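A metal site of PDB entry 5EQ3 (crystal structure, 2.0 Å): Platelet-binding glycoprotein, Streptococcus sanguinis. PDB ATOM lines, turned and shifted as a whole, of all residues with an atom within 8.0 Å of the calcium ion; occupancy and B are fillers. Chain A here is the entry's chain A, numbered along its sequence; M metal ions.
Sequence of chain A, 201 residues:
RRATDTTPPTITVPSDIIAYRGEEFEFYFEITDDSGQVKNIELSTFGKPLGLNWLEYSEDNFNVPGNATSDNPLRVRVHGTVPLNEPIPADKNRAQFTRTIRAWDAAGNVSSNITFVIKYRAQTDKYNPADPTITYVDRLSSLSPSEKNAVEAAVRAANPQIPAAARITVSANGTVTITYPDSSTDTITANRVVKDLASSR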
ATOM      1  N   THR A   4     -20.823  18.487 -10.270  1.00  0.00           N
ATOM      2  CA  THR A   4     -22.164  18.284  -9.741  1.00  0.00           C
ATOM      3  C   THR A   4     -22.390  19.037  -8.419  1.00  0.00           C
ATOM      4  O   THR A   4     -21.453  19.229  -7.628  1.00  0.00           O
ATOM      5  CB  THR A   4     -22.450  16.786  -9.527  1.00  0.00           C
ATOM      6  OG1 THR A   4     -21.511  16.247  -8.580  1.00  0.00           O
ATOM      7  CG2 THR A   4     -22.325  16.036 -10.840  1.00  0.00           C
ATOM      8  N   ASP A   5     -23.624  19.481  -8.193  1.00  0.00           N
ATOM      9  CA  ASP A   5     -23.998  20.192  -6.959  1.00  0.00           C
ATOM     10  C   ASP A   5     -24.195  19.193  -5.826  1.00  0.00           C
ATOM     11  O   ASP A   5     -25.124  18.386  -5.858  1.00  0.00           O
ATOM     12  CB  ASP A   5     -25.292  20.998  -7.185  1.00  0.00           C
ATOM     13  CG  ASP A   5     -25.600  21.991  -6.040  1.00  0.00           C
ATOM     14  OD1 ASP A   5     -25.079  21.866  -4.910  1.00  0.00           O
ATOM     15  OD2 ASP A   5     -26.392  22.916  -6.298  1.00  0.00           O
ATOM     16  N   THR A   6     -23.321  19.266  -4.823  1.00  0.00           N
ATOM     17  CA  THR A   6     -23.443  18.401  -3.654  1.00  0.00           C
ATOM     18  C   THR A   6     -23.623  19.224  -2.382  1.00  0.00           C
ATOM     19  O   THR A   6     -23.587  18.678  -1.275  1.00  0.00           O
ATOM     20  CB  THR A   6     -22.187  17.532  -3.486  1.00  0.00           C
ATOM     21  OG1 THR A   6     -21.058  18.367  -3.226  1.00  0.00           O
ATOM     22  CG2 THR A   6     -21.937  16.692  -4.732  1.00  0.00           C
ATOM     23  N   THR A   7     -23.794  20.527  -2.530  1.00  0.00           N
ATOM     24  CA  THR A   7     -23.806  21.426  -1.374  1.00  0.00           C
ATOM     25  C   THR A   7     -25.215  21.949  -1.120  1.00  0.00           C
ATOM     26  O   THR A   7     -25.802  22.489  -2.035  1.00  0.00           O
ATOM     27  CB  THR A   7     -22.865  22.611  -1.619  1.00  0.00           C
ATOM     28  OG1 THR A   7     -21.565  22.123  -1.989  1.00  0.00           O
ATOM     29  CG2 THR A   7     -22.779  23.478  -0.388  1.00  0.00           C
ATOM     30  N   PRO A   8     -25.735  21.806   0.116  1.00  0.00           N
ATOM     31  CA  PRO A   8     -27.123  22.252   0.325  1.00  0.00           C
ATOM     32  C   PRO A   8     -27.240  23.778   0.484  1.00  0.00           C
ATOM     33  O   PRO A   8     -26.215  24.458   0.610  1.00  0.00           O
ATOM     34  CB  PRO A   8     -27.518  21.518   1.610  1.00  0.00           C
ATOM     35  CG  PRO A   8     -26.249  21.425   2.387  1.00  0.00           C
ATOM     36  CD  PRO A   8     -25.119  21.336   1.363  1.00  0.00           C
ATOM     37  N   PRO A   9     -28.468  24.319   0.450  1.00  0.00           N
ATOM     38  CA  PRO A   9     -28.656  25.760   0.666  1.00  0.00           C
ATOM     39  C   PRO A   9     -28.161  26.256   2.027  1.00  0.00           C
ATOM     40  O   PRO A   9     -28.071  25.488   2.980  1.00  0.00           O
ATOM     41  CB  PRO A   9     -30.191  25.939   0.563  1.00  0.00           C
ATOM     42  CG  PRO A   9     -30.641  24.844  -0.315  1.00  0.00           C
ATOM     43  CD  PRO A   9     -29.705  23.658  -0.002  1.00  0.00           C
ATOM     44  N   THR A  10     -27.923  27.558   2.122  1.00  0.00           N
ATOM     45  CA  THR A  10     -27.508  28.214   3.354  1.00  0.00           C
ATOM     46  C   THR A  10     -28.597  29.173   3.841  1.00  0.00           C
ATOM     47  O   THR A  10     -29.010  30.069   3.090  1.00  0.00           O
ATOM     48  CB  THR A  10     -26.191  28.994   3.141  1.00  0.00           C
ATOM     49  OG1 THR A  10     -25.152  28.060   2.826  1.00  0.00           O
ATOM     50  CG2 THR A  10     -25.807  29.774   4.390  1.00  0.00           C
ATOM     51  N   THR A  32     -29.700  31.238   0.308  1.00  0.00           N
ATOM     52  CA  THR A  32     -28.907  31.234  -0.931  1.00  0.00           C
ATOM     53  C   THR A  32     -28.426  29.824  -1.225  1.00  0.00           C
ATOM     54  O   THR A  32     -28.376  28.979  -0.315  1.00  0.00           O
ATOM     55  CB  THR A  32     -27.675  32.177  -0.827  1.00  0.00           C
ATOM     56  OG1 THR A  32     -26.745  31.640   0.121  1.00  0.00           O
ATOM     57  CG2 THR A  32     -28.081  33.581  -0.394  1.00  0.00           C
ATOM     58  N   ASP A  33     -28.085  29.530  -2.478  1.00  0.00           N
ATOM     59  CA  ASP A  33     -27.502  28.249  -2.822  1.00  0.00           C
ATOM     60  C   ASP A  33     -26.460  28.488  -3.908  1.00  0.00           C
ATOM     61  O   ASP A  33     -26.581  29.444  -4.693  1.00  0.00           O
ATOM     62  CB  ASP A  33     -28.540  27.227  -3.307  1.00  0.00           C
ATOM     63  CG  ASP A  33     -27.931  25.829  -3.562  1.00  0.00           C
ATOM     64  OD1 ASP A  33     -27.648  25.086  -2.601  1.00  0.00           O
ATOM     65  OD2 ASP A  33     -27.712  25.447  -4.743  1.00  0.00           O
ATOM     66  N   ASP A  34     -25.457  27.625  -3.973  1.00  0.00           N
ATOM     67  CA  ASP A  34     -24.414  27.768  -4.982  1.00  0.00           C
ATOM     68  C   ASP A  34     -24.990  27.663  -6.397  1.00  0.00           C
ATOM     69  O   ASP A  34     -24.509  28.320  -7.297  1.00  0.00           O
ATOM     70  CB  ASP A  34     -23.274  26.759  -4.764  1.00  0.00           C
ATOM     71  CG  ASP A  34     -23.733  25.291  -4.715  1.00  0.00           C
ATOM     72  OD1 ASP A  34     -24.833  25.014  -4.166  1.00  0.00           O
ATOM     73  OD2 ASP A  34     -22.963  24.417  -5.198  1.00  0.00           O
ATOM     74  N   SER A  35     -26.035  26.865  -6.588  1.00  0.00           N
ATOM     75  CA  SER A  35     -26.742  26.798  -7.879  1.00  0.00           C
ATOM     76  C   SER A  35     -27.538  28.051  -8.195  1.00  0.00           C
ATOM     77  O   SER A  35     -27.914  28.266  -9.348  1.00  0.00           O
ATOM     78  CB  SER A  35     -27.708  25.629  -7.909  1.00  0.00           C
ATOM     79  OG  SER A  35     -28.812  25.889  -7.067  1.00  0.00           O
ATOM     80  N   GLY A  36     -27.836  28.848  -7.174  1.00  0.00           N
ATOM     81  CA  GLY A  36     -28.666  30.028  -7.341  1.00  0.00           C
ATOM     82  C   GLY A  36     -30.155  29.707  -7.334  1.00  0.00           C
ATOM     83  O   GLY A  36     -30.968  30.585  -7.572  1.00  0.00           O
ATOM     84  N   GLN A  37     -30.495  28.447  -7.079  1.00  0.00           N
ATOM     85  CA  GLN A  37     -31.876  28.020  -7.070  1.00  0.00           C
ATOM     86  C   GLN A  37     -32.230  27.248  -5.815  1.00  0.00           C
ATOM     87  O   GLN A  37     -31.616  26.221  -5.526  1.00  0.00           O
ATOM     88  CB  GLN A  37     -32.169  27.145  -8.281  1.00  0.00           C
ATOM     89  CG  GLN A  37     -33.672  26.917  -8.456  1.00  0.00           C
ATOM     90  CD  GLN A  37     -34.003  26.242  -9.761  1.00  0.00           C
ATOM     91  OE1 GLN A  37     -33.279  26.382 -10.741  1.00  0.00           O
ATOM     92  NE2 GLN A  37     -35.091  25.496  -9.780  1.00  0.00           N
ATOM     93  N   VAL A  38     -33.230  27.738  -5.078  1.00  0.00           N
ATOM     94  CA  VAL A  38     -33.778  27.028  -3.930  1.00  0.00           C
ATOM     95  C   VAL A  38     -35.167  26.527  -4.283  1.00  0.00           C
ATOM     96  O   VAL A  38     -35.982  27.272  -4.841  1.00  0.00           O
ATOM     97  CB  VAL A  38     -33.780  27.909  -2.676  1.00  0.00           C
ATOM     98  CG1 VAL A  38     -34.741  27.375  -1.612  1.00  0.00           C
ATOM     99  CG2 VAL A  38     -32.351  27.998  -2.140  1.00  0.00           C
ATOM    100  N   TRP A 104     -34.249  22.731   0.538  1.00  0.00           N
ATOM    101  CA  TRP A 104     -33.724  21.946  -0.566  1.00  0.00           C
ATOM    102  C   TRP A 104     -33.264  22.844  -1.715  1.00  0.00           C
ATOM    103  O   TRP A 104     -33.865  23.874  -1.956  1.00  0.00           O
ATOM    104  CB  TRP A 104     -34.788  20.989  -1.106  1.00  0.00           C
ATOM    105  CG  TRP A 104     -35.113  19.799  -0.263  1.00  0.00           C
ATOM    106  CD1 TRP A 104     -34.700  18.521  -0.468  1.00  0.00           C
ATOM    107  CD2 TRP A 104     -35.936  19.775   0.912  1.00  0.00           C
ATOM    108  NE1 TRP A 104     -35.230  17.700   0.501  1.00  0.00           N
ATOM    109  CE2 TRP A 104     -35.979  18.441   1.356  1.00  0.00           C
ATOM    110  CE3 TRP A 104     -36.644  20.748   1.608  1.00  0.00           C
ATOM    111  CZ2 TRP A 104     -36.705  18.059   2.494  1.00  0.00           C
ATOM    112  CZ3 TRP A 104     -37.370  20.366   2.746  1.00  0.00           C
ATOM    113  CH2 TRP A 104     -37.395  19.028   3.161  1.00  0.00           C
ATOM    114  N   ASP A 105     -32.248  22.423  -2.452  1.00  0.00           N
ATOM    115  CA  ASP A 105     -31.947  23.063  -3.736  1.00  0.00           C
ATOM    116  C   ASP A 105     -32.579  22.226  -4.852  1.00  0.00           C
ATOM    117  O   ASP A 105     -33.297  21.270  -4.574  1.00  0.00           O
ATOM    118  CB  ASP A 105     -30.424  23.254  -3.937  1.00  0.00           C
ATOM    119  CG  ASP A 105     -29.647  21.929  -3.997  1.00  0.00           C
ATOM    120  OD1 ASP A 105     -30.236  20.861  -4.263  1.00  0.00           O
ATOM    121  OD2 ASP A 105     -28.410  21.952  -3.784  1.00  0.00           O
ATOM    122  N   ALA A 106     -32.317  22.577  -6.105  1.00  0.00           N
ATOM    123  CA  ALA A 106     -32.883  21.841  -7.235  1.00  0.00           C
ATOM    124  C   ALA A 106     -32.213  20.478  -7.455  1.00  0.00           C
ATOM    125  O   ALA A 106     -32.727  19.652  -8.206  1.00  0.00           O
ATOM    126  CB  ALA A 106     -32.771  22.680  -8.503  1.00  0.00           C
ATOM    127  N   ALA A 107     -31.071  20.265  -6.812  1.00  0.00           N
ATOM    128  CA  ALA A 107     -30.306  19.032  -6.983  1.00  0.00           C
ATOM    129  C   ALA A 107     -30.565  17.990  -5.877  1.00  0.00           C
ATOM    130  O   ALA A 107     -29.948  16.929  -5.850  1.00  0.00           O
ATOM    131  CB  ALA A 107     -28.832  19.342  -7.046  1.00  0.00           C
ATOM    132  N   GLY A 108     -31.470  18.295  -4.948  1.00  0.00           N
ATOM    133  CA  GLY A 108     -31.851  17.320  -3.944  1.00  0.00           C
ATOM    134  C   GLY A 108     -30.995  17.330  -2.694  1.00  0.00           C
ATOM    135  O   GLY A 108     -31.076  16.422  -1.859  1.00  0.00           O
ATOM    136  N   ASN A 109     -30.156  18.346  -2.571  1.00  0.00           N
ATOM    137  CA  ASN A 109     -29.398  18.547  -1.350  1.00  0.00           C
ATOM    138  C   ASN A 109     -30.273  19.302  -0.350  1.00  0.00           C
ATOM    139  O   ASN A 109     -30.831  20.352  -0.676  1.00  0.00           O
ATOM    140  CB  ASN A 109     -28.111  19.306  -1.648  1.00  0.00           C
ATOM    141  CG  ASN A 109     -27.280  18.628  -2.709  1.00  0.00           C
ATOM    142  OD1 ASN A 109     -26.764  17.546  -2.482  1.00  0.00           O
ATOM    143  ND2 ASN A 109     -27.129  19.275  -3.862  1.00  0.00           N
ATOM    144  N   VAL A 110     -30.427  18.765   0.854  1.00  0.00           N
ATOM    145  CA  VAL A 110     -31.215  19.455   1.865  1.00  0.00           C
ATOM    146  C   VAL A 110     -30.283  19.921   2.973  1.00  0.00           C
ATOM    147  O   VAL A 110     -29.373  19.206   3.380  1.00  0.00           O
ATOM    148  CB  VAL A 110     -32.350  18.568   2.439  1.00  0.00           C
ATOM    149  CG1 VAL A 110     -31.822  17.347   3.145  1.00  0.00           C
ATOM    150  CG2 VAL A 110     -33.215  19.372   3.405  1.00  0.00           C
HETATM  151 CA    CA M   1     -26.606  23.465  -4.004  1.00  0.00          CA
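Of the 21 residues printed, 5 come within 4 Å of the calcium ion. The nearest printed residue that does not touch the calcium ion is Asn 109 (4.2 Å).
The calcium ion is bound by O of Thr 7, OD1 of Asp 34, OD2 of Asp 105, OD2 of Asp 5, OD1 of Asp 33, OD2 of Asp 33 and OD1 of Asp 5. The calcium ion has seven donor atoms within binding distance.
OD1 of Asp 105 lies within hydrogen-bond range of N of Asn 109 (3.0 Å). OD2 of Asp 33 sits close to OG of Ser 35, at 2.6 Å. The side-chain amide nitrogen (ND2) of Asn 109 sits at hydrogen-bond distance from the backbone carbonyl oxygen (O) of Asp 5. The side-chain carboxylate of Asp 105 lies within hydrogen-bond range of the backbone NH of Ala 107 (2.7 Å). N of Gly 108 is in hydrogen-bond range of OD1 of Asp 105, 2.9 Å away.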
